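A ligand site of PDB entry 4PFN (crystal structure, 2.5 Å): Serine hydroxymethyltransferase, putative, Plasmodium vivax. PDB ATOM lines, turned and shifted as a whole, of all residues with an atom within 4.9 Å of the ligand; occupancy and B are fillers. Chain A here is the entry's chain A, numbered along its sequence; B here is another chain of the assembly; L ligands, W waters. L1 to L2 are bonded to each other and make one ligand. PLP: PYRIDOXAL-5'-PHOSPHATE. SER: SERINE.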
ATOM      1  N   ILE A  32      26.031 -33.545 -26.674  1.00  0.00           N
ATOM      2  CA  ILE A  32      25.562 -32.220 -26.248  1.00  0.00           C
ATOM      3  C   ILE A  32      25.936 -31.194 -27.306  1.00  0.00           C
ATOM      4  O   ILE A  32      27.125 -30.959 -27.566  1.00  0.00           O
ATOM      5  CB  ILE A  32      26.139 -31.775 -24.899  1.00  0.00           C
ATOM      6  CG1 ILE A  32      26.069 -32.890 -23.841  1.00  0.00           C
ATOM      7  CG2 ILE A  32      25.415 -30.506 -24.439  1.00  0.00           C
ATOM      8  CD1 ILE A  32      24.708 -33.131 -23.206  1.00  0.00           C
ATOM      9  N   SER A  34      25.982 -28.113 -27.553  1.00  0.00           N
ATOM     10  CA  SER A  34      26.737 -26.954 -27.119  1.00  0.00           C
ATOM     11  C   SER A  34      28.091 -27.277 -26.493  1.00  0.00           C
ATOM     12  O   SER A  34      28.733 -26.415 -25.902  1.00  0.00           O
ATOM     13  CB  SER A  34      25.919 -26.179 -26.111  1.00  0.00           C
ATOM     14  OG  SER A  34      25.708 -26.969 -24.980  1.00  0.00           O
ATOM     15  N   SER A 100      31.010 -14.795 -20.227  1.00  0.00           N
ATOM     16  CA  SER A 100      30.241 -15.922 -20.746  1.00  0.00           C
ATOM     17  C   SER A 100      29.058 -15.413 -21.581  1.00  0.00           C
ATOM     18  O   SER A 100      28.745 -14.217 -21.578  1.00  0.00           O
ATOM     19  CB  SER A 100      29.761 -16.823 -19.579  1.00  0.00           C
ATOM     20  OG  SER A 100      29.677 -18.190 -19.966  1.00  0.00           O
ATOM     21  N   GLY A 101      28.405 -16.318 -22.299  1.00  0.00           N
ATOM     22  CA  GLY A 101      27.348 -15.910 -23.219  1.00  0.00           C
ATOM     23  C   GLY A 101      26.222 -15.124 -22.587  1.00  0.00           C
ATOM     24  O   GLY A 101      25.689 -14.200 -23.192  1.00  0.00           O
ATOM     25  N   SER A 102      25.834 -15.493 -21.371  1.00  0.00           N
ATOM     26  CA  SER A 102      24.713 -14.868 -20.713  1.00  0.00           C
ATOM     27  C   SER A 102      25.042 -13.421 -20.345  1.00  0.00           C
ATOM     28  O   SER A 102      24.285 -12.498 -20.653  1.00  0.00           O
ATOM     29  CB  SER A 102      24.244 -15.691 -19.502  1.00  0.00           C
ATOM     30  OG  SER A 102      23.755 -16.971 -19.903  1.00  0.00           O
ATOM     31  N   ASN A 105      24.997 -11.290 -23.546  1.00  0.00           N
ATOM     32  CA  ASN A 105      23.664 -10.896 -23.999  1.00  0.00           C
ATOM     33  C   ASN A 105      23.050  -9.833 -23.083  1.00  0.00           C
ATOM     34  O   ASN A 105      22.582  -8.793 -23.564  1.00  0.00           O
ATOM     35  CB  ASN A 105      22.746 -12.117 -24.141  1.00  0.00           C
ATOM     36  CG  ASN A 105      23.166 -13.030 -25.274  1.00  0.00           C
ATOM     37  OD1 ASN A 105      24.078 -12.714 -26.038  1.00  0.00           O
ATOM     38  ND2 ASN A 105      22.489 -14.168 -25.402  1.00  0.00           N
ATOM     39  N   HIS A 129      16.982 -18.897 -25.956  1.00  0.00           N
ATOM     40  CA  HIS A 129      17.805 -18.968 -24.755  1.00  0.00           C
ATOM     41  C   HIS A 129      17.196 -18.159 -23.658  1.00  0.00           C
ATOM     42  O   HIS A 129      16.397 -17.239 -23.912  1.00  0.00           O
ATOM     43  CB  HIS A 129      19.225 -18.473 -25.022  1.00  0.00           C
ATOM     44  CG  HIS A 129      20.159 -18.668 -23.855  1.00  0.00           C
ATOM     45  ND1 HIS A 129      20.597 -17.640 -23.099  1.00  0.00           N
ATOM     46  CD2 HIS A 129      20.732 -19.816 -23.321  1.00  0.00           C
ATOM     47  CE1 HIS A 129      21.402 -18.111 -22.137  1.00  0.00           C
ATOM     48  NE2 HIS A 129      21.488 -19.446 -22.272  1.00  0.00           N
ATOM     49  N   THR A 131      18.524 -15.873 -21.798  1.00  0.00           N
ATOM     50  CA  THR A 131      18.858 -14.449 -21.948  1.00  0.00           C
ATOM     51  C   THR A 131      18.191 -13.784 -23.163  1.00  0.00           C
ATOM     52  O   THR A 131      18.498 -12.641 -23.501  1.00  0.00           O
ATOM     53  CB  THR A 131      20.368 -14.224 -22.022  1.00  0.00           C
ATOM     54  OG1 THR A 131      20.895 -14.974 -23.126  1.00  0.00           O
ATOM     55  CG2 THR A 131      21.041 -14.670 -20.735  1.00  0.00           C
ATOM     56  N   HIS A 132      17.281 -14.502 -23.824  1.00  0.00           N
ATOM     57  CA  HIS A 132      16.513 -13.903 -24.891  1.00  0.00           C
ATOM     58  C   HIS A 132      15.177 -13.392 -24.418  1.00  0.00           C
ATOM     59  O   HIS A 132      14.271 -13.177 -25.222  1.00  0.00           O
ATOM     60  CB  HIS A 132      16.379 -14.837 -26.104  1.00  0.00           C
ATOM     61  CG  HIS A 132      17.703 -15.208 -26.754  1.00  0.00           C
ATOM     62  ND1 HIS A 132      17.793 -16.147 -27.706  1.00  0.00           N
ATOM     63  CD2 HIS A 132      19.005 -14.748 -26.534  1.00  0.00           C
ATOM     64  CE1 HIS A 132      19.071 -16.267 -28.095  1.00  0.00           C
ATOM     65  NE2 HIS A 132      19.819 -15.417 -27.367  1.00  0.00           N
ATOM     66  N   GLY A 181      18.922 -16.312 -33.697  1.00  0.00           N
ATOM     67  CA  GLY A 181      20.085 -17.129 -33.321  1.00  0.00           C
ATOM     68  C   GLY A 181      19.726 -17.804 -32.005  1.00  0.00           C
ATOM     69  O   GLY A 181      19.289 -17.124 -31.067  1.00  0.00           O
ATOM     70  N   TYR A 182      19.887 -19.120 -31.928  1.00  0.00           N
ATOM     71  CA  TYR A 182      19.165 -19.885 -30.908  1.00  0.00           C
ATOM     72  C   TYR A 182      19.940 -20.989 -30.177  1.00  0.00           C
ATOM     73  O   TYR A 182      21.052 -21.365 -30.568  1.00  0.00           O
ATOM     74  CB  TYR A 182      17.859 -20.452 -31.492  1.00  0.00           C
ATOM     75  CG  TYR A 182      17.048 -19.420 -32.253  1.00  0.00           C
ATOM     76  CD1 TYR A 182      16.347 -18.417 -31.596  1.00  0.00           C
ATOM     77  CD2 TYR A 182      16.995 -19.441 -33.651  1.00  0.00           C
ATOM     78  CE1 TYR A 182      15.619 -17.472 -32.291  1.00  0.00           C
ATOM     79  CE2 TYR A 182      16.257 -18.508 -34.358  1.00  0.00           C
ATOM     80  CZ  TYR A 182      15.577 -17.511 -33.681  1.00  0.00           C
ATOM     81  OH  TYR A 182      14.858 -16.568 -34.380  1.00  0.00           O
ATOM     82  N   THR A 183      19.308 -21.485 -29.107  1.00  0.00           N
ATOM     83  CA  THR A 183      19.872 -22.530 -28.276  1.00  0.00           C
ATOM     84  C   THR A 183      19.655 -23.866 -28.944  1.00  0.00           C
ATOM     85  O   THR A 183      20.576 -24.699 -29.005  1.00  0.00           O
ATOM     86  CB  THR A 183      19.212 -22.509 -26.897  1.00  0.00           C
ATOM     87  OG1 THR A 183      19.541 -21.284 -26.246  1.00  0.00           O
ATOM     88  CG2 THR A 183      19.687 -23.677 -26.037  1.00  0.00           C
ATOM     89  N   ASP A 208      22.356 -13.866 -32.008  1.00  0.00           N
ATOM     90  CA  ASP A 208      23.144 -14.701 -31.131  1.00  0.00           C
ATOM     91  C   ASP A 208      23.466 -15.969 -31.898  1.00  0.00           C
ATOM     92  O   ASP A 208      22.608 -16.854 -32.014  1.00  0.00           O
ATOM     93  CB  ASP A 208      22.360 -15.021 -29.850  1.00  0.00           C
ATOM     94  CG  ASP A 208      23.179 -15.810 -28.831  1.00  0.00           C
ATOM     95  OD1 ASP A 208      24.264 -16.318 -29.184  1.00  0.00           O
ATOM     96  OD2 ASP A 208      22.727 -15.898 -27.660  1.00  0.00           O
ATOM     97  N   SER A 210      25.840 -18.210 -31.140  1.00  0.00           N
ATOM     98  CA  SER A 210      26.644 -19.078 -30.259  1.00  0.00           C
ATOM     99  C   SER A 210      26.724 -20.534 -30.709  1.00  0.00           C
ATOM    100  O   SER A 210      27.797 -21.135 -30.716  1.00  0.00           O
ATOM    101  CB  SER A 210      26.129 -19.014 -28.829  1.00  0.00           C
ATOM    102  OG  SER A 210      26.275 -17.720 -28.291  1.00  0.00           O
ATOM    103  N   HIS A 211      25.587 -21.092 -31.114  1.00  0.00           N
ATOM    104  CA  HIS A 211      25.543 -22.478 -31.548  1.00  0.00           C
ATOM    105  C   HIS A 211      26.068 -22.734 -32.927  1.00  0.00           C
ATOM    106  O   HIS A 211      26.519 -23.825 -33.226  1.00  0.00           O
ATOM    107  CB  HIS A 211      24.135 -23.022 -31.405  1.00  0.00           C
ATOM    108  CG  HIS A 211      23.926 -23.796 -30.130  1.00  0.00           C
ATOM    109  ND1 HIS A 211      24.100 -25.130 -30.062  1.00  0.00           N
ATOM    110  CD2 HIS A 211      23.576 -23.383 -28.854  1.00  0.00           C
ATOM    111  CE1 HIS A 211      23.860 -25.537 -28.814  1.00  0.00           C
ATOM    112  NE2 HIS A 211      23.537 -24.474 -28.072  1.00  0.00           N
ATOM    113  N   THR A 234      29.120 -17.172 -27.907  1.00  0.00           N
ATOM    114  CA  THR A 234      30.016 -17.792 -26.939  1.00  0.00           C
ATOM    115  C   THR A 234      31.194 -18.360 -27.715  1.00  0.00           C
ATOM    116  O   THR A 234      31.140 -18.452 -28.928  1.00  0.00           O
ATOM    117  CB  THR A 234      29.337 -18.923 -26.130  1.00  0.00           C
ATOM    118  OG1 THR A 234      28.693 -19.848 -27.015  1.00  0.00           O
ATOM    119  CG2 THR A 234      28.323 -18.359 -25.158  1.00  0.00           C
ATOM    120  N   HIS A 236      32.869 -21.329 -26.432  1.00  0.00           N
ATOM    121  CA  HIS A 236      33.093 -22.699 -25.931  1.00  0.00           C
ATOM    122  C   HIS A 236      32.364 -23.774 -26.680  1.00  0.00           C
ATOM    123  O   HIS A 236      32.625 -24.953 -26.445  1.00  0.00           O
ATOM    124  CB  HIS A 236      32.829 -22.803 -24.427  1.00  0.00           C
ATOM    125  CG  HIS A 236      31.628 -22.028 -23.949  1.00  0.00           C
ATOM    126  ND1 HIS A 236      30.465 -22.620 -23.633  1.00  0.00           N
ATOM    127  CD2 HIS A 236      31.440 -20.657 -23.718  1.00  0.00           C
ATOM    128  CE1 HIS A 236      29.582 -21.690 -23.228  1.00  0.00           C
ATOM    129  NE2 HIS A 236      30.176 -20.503 -23.276  1.00  0.00           N
ATOM    130  N   LYS A 237      31.486 -23.400 -27.599  1.00  0.00           N
ATOM    131  CA  LYS A 237      30.664 -24.391 -28.305  1.00  0.00           C
ATOM    132  C   LYS A 237      31.334 -24.831 -29.605  1.00  0.00           C
ATOM    133  O   LYS A 237      32.467 -25.317 -29.581  1.00  0.00           O
ATOM    134  CB  LYS A 237      29.234 -23.866 -28.549  1.00  0.00           C
ATOM    135  CG  LYS A 237      28.509 -23.390 -27.304  1.00  0.00           C
ATOM    136  CD  LYS A 237      27.120 -22.870 -27.641  1.00  0.00           C
ATOM    137  CE  LYS A 237      26.306 -22.553 -26.395  1.00  0.00           C
ATOM    138  NZ  LYS A 237      26.825 -21.399 -25.617  1.00  0.00           N
ATOM    139  N   ARG A 243      35.572 -20.956 -22.265  1.00  0.00           N
ATOM    140  CA  ARG A 243      34.286 -20.431 -21.879  1.00  0.00           C
ATOM    141  C   ARG A 243      34.401 -18.901 -21.775  1.00  0.00           C
ATOM    142  O   ARG A 243      34.951 -18.339 -20.814  1.00  0.00           O
ATOM    143  CB  ARG A 243      33.757 -21.098 -20.579  1.00  0.00           C
ATOM    144  CG  ARG A 243      33.734 -22.614 -20.608  1.00  0.00           C
ATOM    145  CD  ARG A 243      33.027 -23.242 -19.395  1.00  0.00           C
ATOM    146  NE  ARG A 243      31.580 -23.209 -19.594  1.00  0.00           N
ATOM    147  CZ  ARG A 243      30.871 -24.142 -20.207  1.00  0.00           C
ATOM    148  NH1 ARG A 243      31.441 -25.260 -20.660  1.00  0.00           N
ATOM    149  NH2 ARG A 243      29.572 -23.972 -20.353  1.00  0.00           N
ATOM    150  N   ARG A 371      17.741 -33.118 -27.844  1.00  0.00           N
ATOM    151  CA  ARG A 371      18.646 -32.421 -28.750  1.00  0.00           C
ATOM    152  C   ARG A 371      19.988 -33.132 -28.788  1.00  0.00           C
ATOM    153  O   ARG A 371      20.553 -33.458 -27.759  1.00  0.00           O
ATOM    154  CB  ARG A 371      18.828 -30.955 -28.297  1.00  0.00           C
ATOM    155  CG  ARG A 371      19.866 -30.169 -29.092  1.00  0.00           C
ATOM    156  CD  ARG A 371      20.187 -28.839 -28.423  1.00  0.00           C
ATOM    157  NE  ARG A 371      21.042 -28.991 -27.249  1.00  0.00           N
ATOM    158  CZ  ARG A 371      21.526 -27.983 -26.527  1.00  0.00           C
ATOM    159  NH1 ARG A 371      21.235 -26.731 -26.857  1.00  0.00           N
ATOM    160  NH2 ARG A 371      22.302 -28.226 -25.476  1.00  0.00           N
ATOM    161  N   TYR B  54      28.987 -28.629 -19.654  1.00  0.00           N
ATOM    162  CA  TYR B  54      27.799 -27.830 -19.292  1.00  0.00           C
ATOM    163  C   TYR B  54      27.117 -28.383 -18.028  1.00  0.00           C
ATOM    164  O   TYR B  54      26.781 -29.558 -17.943  1.00  0.00           O
ATOM    165  CB  TYR B  54      26.801 -27.698 -20.459  1.00  0.00           C
ATOM    166  CG  TYR B  54      26.734 -26.291 -21.013  1.00  0.00           C
ATOM    167  CD1 TYR B  54      26.103 -25.269 -20.301  1.00  0.00           C
ATOM    168  CD2 TYR B  54      27.327 -25.970 -22.236  1.00  0.00           C
ATOM    169  CE1 TYR B  54      26.066 -23.971 -20.788  1.00  0.00           C
ATOM    170  CE2 TYR B  54      27.283 -24.685 -22.752  1.00  0.00           C
ATOM    171  CZ  TYR B  54      26.664 -23.688 -22.026  1.00  0.00           C
ATOM    172  OH  TYR B  54      26.626 -22.405 -22.530  1.00  0.00           O
ATOM    173  N   GLU B  56      24.640 -26.336 -15.976  1.00  0.00           N
ATOM    174  CA  GLU B  56      23.602 -25.429 -15.502  1.00  0.00           C
ATOM    175  C   GLU B  56      22.811 -26.086 -14.386  1.00  0.00           C
ATOM    176  O   GLU B  56      22.363 -27.235 -14.496  1.00  0.00           O
ATOM    177  CB  GLU B  56      22.657 -25.047 -16.633  1.00  0.00           C
ATOM    178  CG  GLU B  56      23.282 -24.176 -17.710  1.00  0.00           C
ATOM    179  CD  GLU B  56      22.403 -24.055 -18.931  1.00  0.00           C
ATOM    180  OE1 GLU B  56      22.123 -25.081 -19.592  1.00  0.00           O
ATOM    181  OE2 GLU B  56      21.994 -22.918 -19.247  1.00  0.00           O
ATOM    182  N   TYR B  64      21.362 -31.143 -17.152  1.00  0.00           N
ATOM    183  CA  TYR B  64      21.943 -32.225 -17.925  1.00  0.00           C
ATOM    184  C   TYR B  64      22.587 -33.254 -16.998  1.00  0.00           C
ATOM    185  O   TYR B  64      22.946 -32.945 -15.873  1.00  0.00           O
ATOM    186  CB  TYR B  64      22.969 -31.710 -18.947  1.00  0.00           C
ATOM    187  CG  TYR B  64      22.508 -30.575 -19.851  1.00  0.00           C
ATOM    188  CD1 TYR B  64      21.166 -30.195 -19.925  1.00  0.00           C
ATOM    189  CD2 TYR B  64      23.432 -29.904 -20.666  1.00  0.00           C
ATOM    190  CE1 TYR B  64      20.756 -29.169 -20.765  1.00  0.00           C
ATOM    191  CE2 TYR B  64      23.031 -28.880 -21.510  1.00  0.00           C
ATOM    192  CZ  TYR B  64      21.698 -28.517 -21.559  1.00  0.00           C
ATOM    193  OH  TYR B  64      21.296 -27.500 -22.380  1.00  0.00           O
ATOM    194  N   GLN B 270      23.446 -15.817 -14.842  1.00  0.00           N
ATOM    195  CA  GLN B 270      24.389 -16.695 -15.528  1.00  0.00           C
ATOM    196  C   GLN B 270      23.734 -17.906 -16.203  1.00  0.00           C
ATOM    197  O   GLN B 270      22.543 -18.185 -16.011  1.00  0.00           O
ATOM    198  CB  GLN B 270      25.480 -17.147 -14.544  1.00  0.00           C
ATOM    199  CG  GLN B 270      26.245 -16.002 -13.892  1.00  0.00           C
ATOM    200  CD  GLN B 270      27.564 -16.419 -13.260  1.00  0.00           C
ATOM    201  OE1 GLN B 270      28.376 -15.555 -12.939  1.00  0.00           O
ATOM    202  NE2 GLN B 270      27.781 -17.718 -13.066  1.00  0.00           N
ATOM    203  N   GLY B 271      24.516 -18.603 -17.016  1.00  0.00           N
ATOM    204  CA  GLY B 271      24.142 -19.895 -17.565  1.00  0.00           C
ATOM    205  C   GLY B 271      25.081 -20.964 -17.001  1.00  0.00           C
ATOM    206  O   GLY B 271      25.215 -21.114 -15.778  1.00  0.00           O
ATOM    207  N   GLY B 272      25.748 -21.691 -17.903  1.00  0.00           N
ATOM    208  CA  GLY B 272      26.702 -22.723 -17.502  1.00  0.00           C
ATOM    209  C   GLY B 272      27.697 -22.147 -16.527  1.00  0.00           C
ATOM    210  O   GLY B 272      28.206 -21.042 -16.732  1.00  0.00           O
HETATM  211  N1  PLP L   1      23.310 -18.044 -26.086  1.00  0.00           N
HETATM  212  C2  PLP L   1      22.885 -19.219 -26.595  1.00  0.00           C
HETATM  213  C2A PLP L   1      22.261 -19.263 -27.975  1.00  0.00           C
HETATM  214  C3  PLP L   1      23.017 -20.457 -25.791  1.00  0.00           C
HETATM  215  O3  PLP L   1      22.570 -21.627 -26.320  1.00  0.00           O
HETATM  216  C4  PLP L   1      23.624 -20.365 -24.444  1.00  0.00           C
HETATM  217  C4A PLP L   1      23.763 -21.583 -23.617  1.00  0.00           C
HETATM  218  C5  PLP L   1      24.060 -18.996 -24.037  1.00  0.00           C
HETATM  219  C6  PLP L   1      23.873 -17.920 -24.881  1.00  0.00           C
HETATM  220  C5A PLP L   1      24.693 -18.641 -22.712  1.00  0.00           C
HETATM  221  O4P PLP L   1      25.991 -19.205 -22.582  1.00  0.00           O
HETATM  222  P   PLP L   1      26.641 -19.365 -21.136  1.00  0.00           P
HETATM  223  O1P PLP L   1      26.233 -18.145 -20.331  1.00  0.00           O
HETATM  224  O2P PLP L   1      26.127 -20.699 -20.652  1.00  0.00           O
HETATM  225  O3P PLP L   1      28.077 -19.426 -21.567  1.00  0.00           O
HETATM  226  N   SER L   2      23.346 -22.742 -23.904  1.00  0.00           N
HETATM  227  CA  SER L   2      23.108 -24.045 -23.254  1.00  0.00           C
HETATM  228  C   SER L   2      23.285 -25.126 -24.315  1.00  0.00           C
HETATM  229  O   SER L   2      23.514 -26.316 -23.962  1.00  0.00           O
HETATM  230  CB  SER L   2      21.683 -24.146 -22.721  1.00  0.00           C
HETATM  231  OG  SER L   2      21.255 -22.946 -22.092  1.00  0.00           O
HETATM  232  OXT SER L   2      22.849 -24.953 -25.461  1.00  0.00           O
HETATM  233  O   HOH W   1      23.440 -20.755 -20.546  1.00  0.00           O
HETATM  234  O   HOH W   2      27.285 -18.294 -17.812  1.00  0.00           O
HETATM  235  O   HOH W   3      18.552 -21.767 -22.379  1.00  0.00           O
HETATM  236  O   HOH W   4      29.318 -21.386 -19.397  1.00  0.00           O
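Water W1 lies within hydrogen-bond range of an oxygen (O2P) of PLP L1 (2.7 Å), the side-chain carboxylate of Glu 56 of chain B (2.9 Å) and a ring nitrogen (NE2) of His 129 (2.9 Å). Water W2 lies within hydrogen-bond range of O1P of PLP L1 (2.7 Å), N of Gly 271 of chain B (2.9 Å), O of Gly 272 of chain B (3.1 Å) and OG of Ser 100 (3.2 Å). Water W4 lies within hydrogen-bond range of NH2 of Arg 243 (2.8 Å), O of Gly 272 of chain B (2.9 Å), O3P of PLP L1 (3.2 Å) and OG of Ser 100 (3.3 Å).
CD2 of His 129 touches C4 of PLP L1, at 3.2 Å. O of Tyr 182 touches C2A of PLP L1, at 3.6 Å. Ser 210 touches the ligand. CG2 of Thr 234 touches O4P of PLP L1 (3.6 Å). NZ of Lys 237 touches C4 of PLP L1 (3.6 Å). CA of Gly 271 of chain B touches O2P of PLP L1, 3.8 Å away. Of the 26 residues printed, 19 come within 4 Å of the ligand.
The guanidinium group (NH1) of Arg 371 lies within hydrogen-bond range of a ring nitrogen (NE2) of His 211. NH2 of Arg 371 sits at hydrogen-bond distance from OH of Tyr 64 of chain B (3.3 Å). OD1 of Asp 208 sits at hydrogen-bond distance from OG of Ser 210, at 2.6 Å. The side-chain carboxylate (OD2) of Asp 208 lies within hydrogen-bond range of a ring nitrogen (NE2) of His 132 (3.0 Å). The backbone carbonyl oxygen (O) of Thr 183 sits at hydrogen-bond distance from a ring nitrogen (NE2) of His 211, at 3.1 Å. The side-chain hydroxyl (OG) of Ser 102 is in hydrogen-bond range of the backbone NH (N) of Gly 271 of chain B, 3.4 Å away. N of His 129 is in hydrogen-bond range of ND1 of His 132 (3.4 Å). The backbone NH (N) of Thr 234 sits at hydrogen-bond distance from the side-chain hydroxyl (OG) of Ser 210.
OG of Ser 34 is in hydrogen-bond range of O of SER L2. The side-chain hydroxyl (OG) of Ser 100 lies within hydrogen-bond range of an oxygen (O3P) of PLP L1 (2.6 Å). An oxygen (O2P) of PLP L1 lies within hydrogen-bond range of the side-chain hydroxyl (OH) of Tyr 54 of chain B (2.6 Å). An oxygen (O) of SER L2 is in salt-bridge range of the guanidinium group (NH2) of Arg 371 (2.7 Å). OD2 of Asp 208 lies within hydrogen-bond range of N1 of PLP L1 (2.7 Å). A ring nitrogen (NE2) of His 211 is in hydrogen-bond range of an oxygen (OXT) of SER L2, at 2.7 Å. The backbone NH (N) of Ser 102 is in hydrogen-bond range of an oxygen (O1P) of PLP L1. An oxygen (O1P) of PLP L1 sits at hydrogen-bond distance from the side-chain hydroxyl (OG) of Ser 102. NE2 of His 236 sits at hydrogen-bond distance from O3P of PLP L1 (2.9 Å). The side-chain carboxylate (OE2) of Glu 56 of chain B lies within hydrogen-bond range of an oxygen (OG) of SER L2. An oxygen (O2P) of PLP L1 sits at hydrogen-bond distance from the backbone NH (N) of Gly 272 of chain B (2.9 Å). OH of Tyr 64 of chain B sits at hydrogen-bond distance from O of SER L2, at 3.0 Å. The side-chain hydroxyl (OG1) of Thr 183 is in hydrogen-bond range of an oxygen (O3) of PLP L1, 3.0 Å away. An oxygen (O3P) of PLP L1 lies within hydrogen-bond range of the backbone NH (N) of Gly 101.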
